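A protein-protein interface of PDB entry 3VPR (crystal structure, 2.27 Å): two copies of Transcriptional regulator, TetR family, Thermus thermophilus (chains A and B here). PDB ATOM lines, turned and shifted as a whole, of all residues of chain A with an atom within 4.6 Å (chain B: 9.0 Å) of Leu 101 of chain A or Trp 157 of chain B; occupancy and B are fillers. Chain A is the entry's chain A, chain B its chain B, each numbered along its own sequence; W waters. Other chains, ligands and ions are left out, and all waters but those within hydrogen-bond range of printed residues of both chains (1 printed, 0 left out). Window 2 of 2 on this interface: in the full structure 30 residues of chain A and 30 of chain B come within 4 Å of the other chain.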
ATOM      1  N   PHE A  97      -5.758 -11.821   2.105  1.00  0.00           N
ATOM      2  CA  PHE A  97      -4.721 -11.351   1.196  1.00  0.00           C
ATOM      3  C   PHE A  97      -3.360 -11.337   1.863  1.00  0.00           C
ATOM      4  O   PHE A  97      -2.362 -11.704   1.245  1.00  0.00           O
ATOM      5  CB  PHE A  97      -5.087  -9.970   0.665  1.00  0.00           C
ATOM      6  CG  PHE A  97      -6.078 -10.016  -0.455  1.00  0.00           C
ATOM      7  CD1 PHE A  97      -5.649 -10.125  -1.776  1.00  0.00           C
ATOM      8  CD2 PHE A  97      -7.438 -10.038  -0.192  1.00  0.00           C
ATOM      9  CE1 PHE A  97      -6.566 -10.257  -2.816  1.00  0.00           C
ATOM     10  CE2 PHE A  97      -8.360 -10.171  -1.226  1.00  0.00           C
ATOM     11  CZ  PHE A  97      -7.924 -10.282  -2.538  1.00  0.00           C
ATOM     12  N   VAL A  98      -3.319 -10.921   3.124  1.00  0.00           N
ATOM     13  CA  VAL A  98      -2.063 -10.903   3.853  1.00  0.00           C
ATOM     14  C   VAL A  98      -1.569 -12.343   3.980  1.00  0.00           C
ATOM     15  O   VAL A  98      -0.371 -12.614   3.911  1.00  0.00           O
ATOM     16  CB  VAL A  98      -2.238 -10.282   5.255  1.00  0.00           C
ATOM     17  CG1 VAL A  98      -0.941 -10.427   6.062  1.00  0.00           C
ATOM     18  CG2 VAL A  98      -2.617  -8.810   5.119  1.00  0.00           C
ATOM     19  N   THR A  99      -2.500 -13.275   4.137  1.00  0.00           N
ATOM     20  CA  THR A  99      -2.129 -14.679   4.274  1.00  0.00           C
ATOM     21  C   THR A  99      -1.591 -15.234   2.957  1.00  0.00           C
ATOM     22  O   THR A  99      -0.522 -15.847   2.919  1.00  0.00           O
ATOM     23  CB  THR A  99      -3.336 -15.543   4.717  1.00  0.00           C
ATOM     24  OG1 THR A  99      -3.766 -15.139   6.024  1.00  0.00           O
ATOM     25  CG2 THR A  99      -2.953 -17.020   4.749  1.00  0.00           C
ATOM     26  N   MET A 100      -2.342 -15.017   1.884  1.00  0.00           N
ATOM     27  CA  MET A 100      -1.962 -15.500   0.561  1.00  0.00           C
ATOM     28  C   MET A 100      -0.596 -15.020   0.050  1.00  0.00           C
ATOM     29  O   MET A 100       0.215 -15.817  -0.427  1.00  0.00           O
ATOM     30  CB  MET A 100      -3.019 -15.099  -0.465  1.00  0.00           C
ATOM     31  CG  MET A 100      -2.540 -15.334  -1.880  1.00  0.00           C
ATOM     32  SD  MET A 100      -3.278 -14.095  -3.125  1.00  0.00           S
ATOM     33  CE  MET A 100      -2.336 -12.503  -2.567  1.00  0.00           C
ATOM     34  N   LEU A 101      -0.360 -13.715   0.133  1.00  0.00           N
ATOM     35  CA  LEU A 101       0.886 -13.127  -0.339  1.00  0.00           C
ATOM     36  C   LEU A 101       2.128 -13.777   0.261  1.00  0.00           C
ATOM     37  O   LEU A 101       3.011 -14.238  -0.463  1.00  0.00           O
ATOM     38  CB  LEU A 101       0.903 -11.624  -0.035  1.00  0.00           C
ATOM     39  CG  LEU A 101       2.032 -10.814  -0.680  1.00  0.00           C
ATOM     40  CD1 LEU A 101       1.907 -10.908  -2.192  1.00  0.00           C
ATOM     41  CD2 LEU A 101       1.965  -9.354  -0.234  1.00  0.00           C
ATOM     42  N   GLN A 102       2.189 -13.824   1.585  1.00  0.00           N
ATOM     43  CA  GLN A 102       3.341 -14.393   2.270  1.00  0.00           C
ATOM     44  C   GLN A 102       3.476 -15.906   2.110  1.00  0.00           C
ATOM     45  O   GLN A 102       4.583 -16.429   1.981  1.00  0.00           O
ATOM     46  CB  GLN A 102       3.286 -14.044   3.767  1.00  0.00           C
ATOM     47  CG  GLN A 102       2.177 -14.750   4.533  1.00  0.00           C
ATOM     48  CD  GLN A 102       2.198 -14.452   6.028  1.00  0.00           C
ATOM     49  OE1 GLN A 102       3.205 -14.667   6.706  1.00  0.00           O
ATOM     50  NE2 GLN A 102       1.078 -13.962   6.546  1.00  0.00           N
ATOM     51  N   GLY A 103       2.343 -16.601   2.101  1.00  0.00           N
ATOM     52  CA  GLY A 103       2.363 -18.052   2.012  1.00  0.00           C
ATOM     53  C   GLY A 103       2.757 -18.742   0.720  1.00  0.00           C
ATOM     54  O   GLY A 103       3.062 -19.933   0.745  1.00  0.00           O
ATOM     55  N   ILE A 104       2.766 -18.016  -0.394  1.00  0.00           N
ATOM     56  CA  ILE A 104       3.095 -18.600  -1.696  1.00  0.00           C
ATOM     57  C   ILE A 104       4.117 -19.746  -1.708  1.00  0.00           C
ATOM     58  O   ILE A 104       3.821 -20.840  -2.195  1.00  0.00           O
ATOM     59  CB  ILE A 104       3.569 -17.513  -2.701  1.00  0.00           C
ATOM     60  CG1 ILE A 104       3.793 -18.137  -4.083  1.00  0.00           C
ATOM     61  CG2 ILE A 104       4.846 -16.851  -2.203  1.00  0.00           C
ATOM     62  CD1 ILE A 104       2.530 -18.688  -4.723  1.00  0.00           C
ATOM     63  N   SER A 153       0.309  -3.493 -10.134  1.00  0.00           N
ATOM     64  CA  SER A 153       1.298  -3.049  -9.159  1.00  0.00           C
ATOM     65  C   SER A 153       0.670  -2.009  -8.232  1.00  0.00           C
ATOM     66  O   SER A 153       0.861  -2.052  -7.020  1.00  0.00           O
ATOM     67  CB  SER A 153       2.530  -2.450  -9.856  1.00  0.00           C
ATOM     68  OG  SER A 153       3.199  -3.435 -10.631  1.00  0.00           O
ATOM     69  N   ASN A 156      -2.028  -4.130  -6.066  1.00  0.00           N
ATOM     70  CA  ASN A 156      -1.426  -5.106  -5.149  1.00  0.00           C
ATOM     71  C   ASN A 156      -0.436  -4.532  -4.140  1.00  0.00           C
ATOM     72  O   ASN A 156      -0.378  -5.007  -3.009  1.00  0.00           O
ATOM     73  CB  ASN A 156      -0.767  -6.258  -5.920  1.00  0.00           C
ATOM     74  CG  ASN A 156      -1.777  -7.093  -6.691  1.00  0.00           C
ATOM     75  OD1 ASN A 156      -2.959  -7.088  -6.360  1.00  0.00           O
ATOM     76  ND2 ASN A 156      -1.316  -7.818  -7.716  1.00  0.00           N
ATOM     77  N   TRP A 157       0.340  -3.522  -4.526  1.00  0.00           N
ATOM     78  CA  TRP A 157       1.278  -2.930  -3.577  1.00  0.00           C
ATOM     79  C   TRP A 157       0.516  -2.382  -2.370  1.00  0.00           C
ATOM     80  O   TRP A 157       1.090  -2.236  -1.297  1.00  0.00           O
ATOM     81  CB  TRP A 157       2.087  -1.804  -4.221  1.00  0.00           C
ATOM     82  CG  TRP A 157       3.234  -1.292  -3.363  1.00  0.00           C
ATOM     83  CD1 TRP A 157       3.460   0.005  -2.972  1.00  0.00           C
ATOM     84  CD2 TRP A 157       4.343  -2.053  -2.867  1.00  0.00           C
ATOM     85  NE1 TRP A 157       4.639   0.093  -2.270  1.00  0.00           N
ATOM     86  CE2 TRP A 157       5.199  -1.153  -2.190  1.00  0.00           C
ATOM     87  CE3 TRP A 157       4.696  -3.407  -2.929  1.00  0.00           C
ATOM     88  CZ2 TRP A 157       6.391  -1.566  -1.584  1.00  0.00           C
ATOM     89  CZ3 TRP A 157       5.884  -3.820  -2.324  1.00  0.00           C
ATOM     90  CH2 TRP A 157       6.715  -2.899  -1.658  1.00  0.00           C
ATOM     91  N   ILE A 159      -1.329  -3.817  -0.498  1.00  0.00           N
ATOM     92  CA  ILE A 159      -1.249  -4.846   0.540  1.00  0.00           C
ATOM     93  C   ILE A 159      -0.134  -4.539   1.545  1.00  0.00           C
ATOM     94  O   ILE A 159      -0.110  -5.092   2.643  1.00  0.00           O
ATOM     95  CB  ILE A 159      -0.990  -6.252  -0.093  1.00  0.00           C
ATOM     96  CG1 ILE A 159      -2.168  -6.637  -1.002  1.00  0.00           C
ATOM     97  CG2 ILE A 159      -0.787  -7.311   1.001  1.00  0.00           C
ATOM     98  CD1 ILE A 159      -1.909  -7.860  -1.887  1.00  0.00           C
ATOM     99  N   HIS B  86      16.280   4.461 -10.022  1.00  0.00           N
ATOM    100  CA  HIS B  86      15.731   3.525  -9.050  1.00  0.00           C
ATOM    101  C   HIS B  86      15.795   2.097  -9.588  1.00  0.00           C
ATOM    102  O   HIS B  86      16.353   1.201  -8.943  1.00  0.00           O
ATOM    103  CB  HIS B  86      14.283   3.908  -8.727  1.00  0.00           C
ATOM    104  CG  HIS B  86      13.605   2.982  -7.763  1.00  0.00           C
ATOM    105  ND1 HIS B  86      12.990   3.427  -6.613  1.00  0.00           N
ATOM    106  CD2 HIS B  86      13.419   1.641  -7.793  1.00  0.00           C
ATOM    107  CE1 HIS B  86      12.455   2.402  -5.977  1.00  0.00           C
ATOM    108  NE2 HIS B  86      12.699   1.307  -6.674  1.00  0.00           N
ATOM    109  N   PHE B  90      18.195  -0.941  -8.475  1.00  0.00           N
ATOM    110  CA  PHE B  90      17.533  -2.147  -8.017  1.00  0.00           C
ATOM    111  C   PHE B  90      18.122  -3.377  -8.712  1.00  0.00           C
ATOM    112  O   PHE B  90      18.421  -4.382  -8.069  1.00  0.00           O
ATOM    113  CB  PHE B  90      16.029  -2.042  -8.291  1.00  0.00           C
ATOM    114  CG  PHE B  90      15.340  -3.368  -8.439  1.00  0.00           C
ATOM    115  CD1 PHE B  90      15.188  -4.225  -7.351  1.00  0.00           C
ATOM    116  CD2 PHE B  90      14.833  -3.755  -9.672  1.00  0.00           C
ATOM    117  CE1 PHE B  90      14.533  -5.458  -7.494  1.00  0.00           C
ATOM    118  CE2 PHE B  90      14.178  -4.980  -9.826  1.00  0.00           C
ATOM    119  CZ  PHE B  90      14.025  -5.833  -8.743  1.00  0.00           C
ATOM    120  N   LEU B 101      13.797  -7.776   1.905  1.00  0.00           N
ATOM    121  CA  LEU B 101      12.377  -8.093   1.916  1.00  0.00           C
ATOM    122  C   LEU B 101      12.086  -9.334   2.754  1.00  0.00           C
ATOM    123  O   LEU B 101      10.983  -9.507   3.262  1.00  0.00           O
ATOM    124  CB  LEU B 101      11.883  -8.304   0.483  1.00  0.00           C
ATOM    125  CG  LEU B 101      10.371  -8.381   0.251  1.00  0.00           C
ATOM    126  CD1 LEU B 101       9.829  -9.748   0.637  1.00  0.00           C
ATOM    127  CD2 LEU B 101       9.694  -7.265   1.048  1.00  0.00           C
ATOM    128  N   ARG B 149       2.958   7.500  -4.576  1.00  0.00           N
ATOM    129  CA  ARG B 149       2.745   6.131  -4.142  1.00  0.00           C
ATOM    130  C   ARG B 149       2.537   5.248  -5.365  1.00  0.00           C
ATOM    131  O   ARG B 149       2.943   4.083  -5.386  1.00  0.00           O
ATOM    132  CB  ARG B 149       1.518   6.053  -3.233  1.00  0.00           C
ATOM    133  CG  ARG B 149       1.281   4.677  -2.642  1.00  0.00           C
ATOM    134  CD  ARG B 149       2.232   4.420  -1.508  1.00  0.00           C
ATOM    135  NE  ARG B 149       2.217   5.550  -0.590  1.00  0.00           N
ATOM    136  CZ  ARG B 149       2.537   5.479   0.696  1.00  0.00           C
ATOM    137  NH1 ARG B 149       2.894   4.322   1.230  1.00  0.00           N
ATOM    138  NH2 ARG B 149       2.508   6.574   1.442  1.00  0.00           N
ATOM    139  N   ALA B 150       1.896   5.814  -6.386  1.00  0.00           N
ATOM    140  CA  ALA B 150       1.618   5.071  -7.602  1.00  0.00           C
ATOM    141  C   ALA B 150       2.922   4.728  -8.315  1.00  0.00           C
ATOM    142  O   ALA B 150       3.146   3.572  -8.698  1.00  0.00           O
ATOM    143  CB  ALA B 150       0.695   5.878  -8.516  1.00  0.00           C
ATOM    144  N   VAL B 151       3.777   5.733  -8.476  1.00  0.00           N
ATOM    145  CA  VAL B 151       5.069   5.558  -9.135  1.00  0.00           C
ATOM    146  C   VAL B 151       5.914   4.529  -8.377  1.00  0.00           C
ATOM    147  O   VAL B 151       6.447   3.597  -8.973  1.00  0.00           O
ATOM    148  CB  VAL B 151       5.810   6.909  -9.208  1.00  0.00           C
ATOM    149  CG1 VAL B 151       7.283   6.710  -9.591  1.00  0.00           C
ATOM    150  CG2 VAL B 151       5.112   7.794 -10.224  1.00  0.00           C
ATOM    151  N   LEU B 152       6.009   4.698  -7.060  1.00  0.00           N
ATOM    152  CA  LEU B 152       6.768   3.783  -6.205  1.00  0.00           C
ATOM    153  C   LEU B 152       6.188   2.357  -6.223  1.00  0.00           C
ATOM    154  O   LEU B 152       6.924   1.374  -6.102  1.00  0.00           O
ATOM    155  CB  LEU B 152       6.821   4.330  -4.769  1.00  0.00           C
ATOM    156  CG  LEU B 152       7.760   5.534  -4.609  1.00  0.00           C
ATOM    157  CD1 LEU B 152       7.805   5.987  -3.160  1.00  0.00           C
ATOM    158  CD2 LEU B 152       9.166   5.143  -5.061  1.00  0.00           C
ATOM    159  N   SER B 153       4.873   2.241  -6.382  1.00  0.00           N
ATOM    160  CA  SER B 153       4.246   0.926  -6.442  1.00  0.00           C
ATOM    161  C   SER B 153       4.736   0.204  -7.691  1.00  0.00           C
ATOM    162  O   SER B 153       5.056  -0.980  -7.652  1.00  0.00           O
ATOM    163  CB  SER B 153       2.721   1.061  -6.482  1.00  0.00           C
ATOM    164  OG  SER B 153       2.258   1.706  -5.314  1.00  0.00           O
ATOM    165  N   MET B 154       4.793   0.930  -8.801  1.00  0.00           N
ATOM    166  CA  MET B 154       5.261   0.373 -10.061  1.00  0.00           C
ATOM    167  C   MET B 154       6.724  -0.082  -9.980  1.00  0.00           C
ATOM    168  O   MET B 154       7.094  -1.135 -10.508  1.00  0.00           O
ATOM    169  CB  MET B 154       5.125   1.418 -11.173  1.00  0.00           C
ATOM    170  CG  MET B 154       3.692   1.643 -11.680  1.00  0.00           C
ATOM    171  SD  MET B 154       3.622   3.109 -12.968  1.00  0.00           S
ATOM    172  CE  MET B 154       2.666   4.361 -11.866  1.00  0.00           C
ATOM    173  N   LEU B 155       7.560   0.722  -9.327  1.00  0.00           N
ATOM    174  CA  LEU B 155       8.973   0.377  -9.214  1.00  0.00           C
ATOM    175  C   LEU B 155       9.204  -0.724  -8.175  1.00  0.00           C
ATOM    176  O   LEU B 155       9.886  -1.716  -8.453  1.00  0.00           O
ATOM    177  CB  LEU B 155       9.797   1.618  -8.841  1.00  0.00           C
ATOM    178  CG  LEU B 155       9.713   2.812  -9.799  1.00  0.00           C
ATOM    179  CD1 LEU B 155      10.239   4.073  -9.111  1.00  0.00           C
ATOM    180  CD2 LEU B 155      10.517   2.519 -11.056  1.00  0.00           C
ATOM    181  N   ASN B 156       8.620  -0.558  -6.986  1.00  0.00           N
ATOM    182  CA  ASN B 156       8.822  -1.528  -5.922  1.00  0.00           C
ATOM    183  C   ASN B 156       8.230  -2.909  -6.142  1.00  0.00           C
ATOM    184  O   ASN B 156       8.823  -3.912  -5.712  1.00  0.00           O
ATOM    185  CB  ASN B 156       8.340  -0.967  -4.590  1.00  0.00           C
ATOM    186  CG  ASN B 156       9.255   0.136  -4.064  1.00  0.00           C
ATOM    187  OD1 ASN B 156      10.320   0.375  -4.613  1.00  0.00           O
ATOM    188  ND2 ASN B 156       8.839   0.802  -3.001  1.00  0.00           N
ATOM    189  N   TRP B 157       7.084  -2.973  -6.817  1.00  0.00           N
ATOM    190  CA  TRP B 157       6.441  -4.254  -7.060  1.00  0.00           C
ATOM    191  C   TRP B 157       7.249  -5.065  -8.062  1.00  0.00           C
ATOM    192  O   TRP B 157       7.005  -6.257  -8.246  1.00  0.00           O
ATOM    193  CB  TRP B 157       5.010  -4.051  -7.563  1.00  0.00           C
ATOM    194  CG  TRP B 157       4.177  -5.301  -7.564  1.00  0.00           C
ATOM    195  CD1 TRP B 157       3.725  -5.989  -8.657  1.00  0.00           C
ATOM    196  CD2 TRP B 157       3.689  -6.011  -6.414  1.00  0.00           C
ATOM    197  NE1 TRP B 157       2.983  -7.079  -8.257  1.00  0.00           N
ATOM    198  CE2 TRP B 157       2.944  -7.118  -6.888  1.00  0.00           C
ATOM    199  CE3 TRP B 157       3.808  -5.818  -5.029  1.00  0.00           C
ATOM    200  CZ2 TRP B 157       2.321  -8.032  -6.027  1.00  0.00           C
ATOM    201  CZ3 TRP B 157       3.188  -6.729  -4.170  1.00  0.00           C
ATOM    202  CH2 TRP B 157       2.451  -7.824  -4.678  1.00  0.00           C
ATOM    203  N   MET B 158       8.218  -4.421  -8.702  1.00  0.00           N
ATOM    204  CA  MET B 158       9.066  -5.112  -9.681  1.00  0.00           C
ATOM    205  C   MET B 158       9.834  -6.270  -9.034  1.00  0.00           C
ATOM    206  O   MET B 158      10.174  -7.249  -9.699  1.00  0.00           O
ATOM    207  CB  MET B 158      10.071  -4.143 -10.318  1.00  0.00           C
ATOM    208  CG  MET B 158       9.536  -3.326 -11.497  1.00  0.00           C
ATOM    209  SD  MET B 158      10.933  -2.203 -12.314  1.00  0.00           S
ATOM    210  CE  MET B 158      11.789  -3.572 -13.386  1.00  0.00           C
ATOM    211  N   ILE B 159      10.108  -6.149  -7.739  1.00  0.00           N
ATOM    212  CA  ILE B 159      10.840  -7.180  -7.011  1.00  0.00           C
ATOM    213  C   ILE B 159      10.061  -8.501  -7.038  1.00  0.00           C
ATOM    214  O   ILE B 159      10.626  -9.583  -6.855  1.00  0.00           O
ATOM    215  CB  ILE B 159      11.095  -6.724  -5.551  1.00  0.00           C
ATOM    216  CG1 ILE B 159      11.888  -5.408  -5.573  1.00  0.00           C
ATOM    217  CG2 ILE B 159      11.884  -7.779  -4.781  1.00  0.00           C
ATOM    218  CD1 ILE B 159      12.224  -4.830  -4.206  1.00  0.00           C
ATOM    219  N   ARG B 160       8.764  -8.403  -7.302  1.00  0.00           N
ATOM    220  CA  ARG B 160       7.904  -9.577  -7.344  1.00  0.00           C
ATOM    221  C   ARG B 160       7.823 -10.283  -8.695  1.00  0.00           C
ATOM    222  O   ARG B 160       7.231 -11.357  -8.792  1.00  0.00           O
ATOM    223  CB  ARG B 160       6.485  -9.208  -6.908  1.00  0.00           C
ATOM    224  CG  ARG B 160       6.149  -9.598  -5.488  1.00  0.00           C
ATOM    225  CD  ARG B 160       6.419  -8.489  -4.505  1.00  0.00           C
ATOM    226  NE  ARG B 160       6.069  -8.917  -3.155  1.00  0.00           N
ATOM    227  CZ  ARG B 160       5.968  -8.103  -2.110  1.00  0.00           C
ATOM    228  NH1 ARG B 160       6.191  -6.801  -2.253  1.00  0.00           N
ATOM    229  NH2 ARG B 160       5.635  -8.591  -0.921  1.00  0.00           N
ATOM    230  N   TRP B 161       8.395  -9.706  -9.742  1.00  0.00           N
ATOM    231  CA  TRP B 161       8.300 -10.365 -11.033  1.00  0.00           C
ATOM    232  C   TRP B 161       9.490 -10.188 -11.966  1.00  0.00           C
ATOM    233  O   TRP B 161       9.687 -10.991 -12.877  1.00  0.00           O
ATOM    234  CB  TRP B 161       7.034  -9.907 -11.751  1.00  0.00           C
ATOM    235  CG  TRP B 161       7.040  -8.455 -12.078  1.00  0.00           C
ATOM    236  CD1 TRP B 161       6.538  -7.439 -11.316  1.00  0.00           C
ATOM    237  CD2 TRP B 161       7.569  -7.848 -13.263  1.00  0.00           C
ATOM    238  NE1 TRP B 161       6.715  -6.238 -11.956  1.00  0.00           N
ATOM    239  CE2 TRP B 161       7.346  -6.457 -13.152  1.00  0.00           C
ATOM    240  CE3 TRP B 161       8.208  -8.343 -14.411  1.00  0.00           C
ATOM    241  CZ2 TRP B 161       7.739  -5.552 -14.147  1.00  0.00           C
ATOM    242  CZ3 TRP B 161       8.600  -7.439 -15.405  1.00  0.00           C
ATOM    243  CH2 TRP B 161       8.360  -6.060 -15.263  1.00  0.00           C
ATOM    244  N   PHE B 162      10.278  -9.141 -11.764  1.00  0.00           N
ATOM    245  CA  PHE B 162      11.417  -8.934 -12.634  1.00  0.00           C
ATOM    246  C   PHE B 162      12.401 -10.097 -12.538  1.00  0.00           C
ATOM    247  O   PHE B 162      12.687 -10.597 -11.449  1.00  0.00           O
ATOM    248  CB  PHE B 162      12.134  -7.631 -12.291  1.00  0.00           C
ATOM    249  CG  PHE B 162      13.368  -7.402 -13.113  1.00  0.00           C
ATOM    250  CD1 PHE B 162      13.268  -7.080 -14.457  1.00  0.00           C
ATOM    251  CD2 PHE B 162      14.630  -7.556 -12.554  1.00  0.00           C
ATOM    252  CE1 PHE B 162      14.407  -6.916 -15.239  1.00  0.00           C
ATOM    253  CE2 PHE B 162      15.775  -7.396 -13.328  1.00  0.00           C
ATOM    254  CZ  PHE B 162      15.660  -7.074 -14.677  1.00  0.00           C
ATOM    255  N   VAL B 173      12.167  -1.105 -18.493  1.00  0.00           N
ATOM    256  CA  VAL B 173      10.841  -1.298 -17.914  1.00  0.00           C
ATOM    257  C   VAL B 173      10.398   0.018 -17.287  1.00  0.00           C
ATOM    258  O   VAL B 173       9.257   0.453 -17.475  1.00  0.00           O
ATOM    259  CB  VAL B 173      10.844  -2.389 -16.805  1.00  0.00           C
ATOM    260  CG1 VAL B 173       9.530  -2.347 -16.028  1.00  0.00           C
ATOM    261  CG2 VAL B 173      11.023  -3.774 -17.431  1.00  0.00           C
ATOM    262  N   TYR B 177       7.256   2.618 -17.950  1.00  0.00           N
ATOM    263  CA  TYR B 177       6.320   2.990 -16.897  1.00  0.00           C
ATOM    264  C   TYR B 177       6.182   4.508 -16.863  1.00  0.00           C
ATOM    265  O   TYR B 177       5.089   5.027 -16.613  1.00  0.00           O
ATOM    266  CB  TYR B 177       6.799   2.507 -15.526  1.00  0.00           C
ATOM    267  CG  TYR B 177       6.521   1.051 -15.221  1.00  0.00           C
ATOM    268  CD1 TYR B 177       5.492   0.367 -15.857  1.00  0.00           C
ATOM    269  CD2 TYR B 177       7.229   0.390 -14.216  1.00  0.00           C
ATOM    270  CE1 TYR B 177       5.155  -0.945 -15.491  1.00  0.00           C
ATOM    271  CE2 TYR B 177       6.912  -0.917 -13.843  1.00  0.00           C
ATOM    272  CZ  TYR B 177       5.871  -1.576 -14.478  1.00  0.00           C
ATOM    273  OH  TYR B 177       5.514  -2.844 -14.066  1.00  0.00           O
HETATM  274  O   HOH W   1       6.033  -3.387 -11.532  1.00  0.00           O
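Water W1 lies within hydrogen-bond range of the side-chain hydroxyl (OH) of Tyr 177 of chain B (2.6 Å), the backbone carbonyl oxygen (O) of Met 154 of chain B (2.7 Å), the indole nitrogen (NE1) of Trp 161 of chain B (3.0 Å) and the side-chain hydroxyl (OG) of Ser 153 of chain A (3.0 Å).
Leu 101 of chain A touches Trp 157 of chain B, but with the chains exchanged Trp 157 of chain A does not touch Leu 101 of chain B (5.9 Å).
Ser 153 of chain A touches Trp 157 of chain B, and with the chains exchanged Trp 157 of chain A touches Ser 153 of chain B.
Asn 156 of chain A touches Trp 157 of chain B, and with the chains exchanged Trp 157 of chain A touches Asn 156 of chain B.
Trp 157 of chain B touches its own counterpart, Trp 157 of chain A.
Hydrophobic or aromatic side chains of chain B within 4 Å of the printed part of chain A: Trp 157.
Hydrophobic or aromatic side chains of chain A that line the printed part of chain B: Leu 101 and Trp 157.
Among the printed residues, 10 pairs touch across the chains.
Among the printed residues, no Asp or Glu carboxylate lies within 4 Å of a Lys or Arg side-chain nitrogen of the other chain.
The side-chain amide oxygen (OD1) of Asn 156 of chain B sits close to a ring nitrogen (NE2) of His 86 of chain B.
O of Arg 149 of chain B sits at hydrogen-bond distance from OG of Ser 153 of chain B, 2.5 Å away.
Leu 101 of chain A touches Trp 157 of chain B (CD1 to CH2, 3.998 Å).
Leu 101 of chain A touches Arg 160 of chain B.
Ser 153 of chain A touches Ser 153 of chain B (CB to O, 3.7 Å).
CB of Ser 153 of chain A touches CA of Met 154 of chain B (3.9 Å).
Trp 157 of chain B touches Ser 153 of chain A (CD1 to OG, 3.3 Å).
CB of Asn 156 of chain A touches CZ2 of Trp 157 of chain B, 3.6 Å away.
OG of Ser 153 of chain B touches CD1 of Trp 157 of chain A, 3.1 Å away.
CZ2 of Trp 157 of chain A touches CB of Asn 156 of chain B, at 3.6 Å.
Trp 157 of chain A touches Trp 157 of chain B.
Arg 160 of chain B touches Trp 157 of chain A (NH1 to CZ3, 3.0 Å).
Of the printed residues of chain B, Leu 101 of chain A touches Trp 157 (3.998 Å) and Arg 160 (3.8 Å).
Ser 153 of chain A touches three residues of chain B.
Of the printed residues of chain B, Trp 157 of chain A touches Ser 153 (3.1 Å), Asn 156 (3.6 Å), Trp 157 (3.3 Å) and Arg 160 (3.0 Å).
Ile 159 of chain A touches none of the printed residues of chain B.
Printed residues of chain A within 4 Å of Asn 156 of chain B: Trp 157 (3.6 Å).
Printed residues of chain A within 4 Å of Trp 157 of chain B: Leu 101 (3.998 Å), Ser 153 (3.3 Å), Asn 156 (3.6 Å) and Trp 157 (3.3 Å).
Phe 162 of chain B touches none of the printed residues of chain A.
The nearest printed residue of chain A that does not touch Trp 157 of chain B is Ile 159 of chain A (5.2 Å).
The nearest printed residue of chain A that does not touch Ser 153 of chain B is Asn 156 of chain A (6.8 Å).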
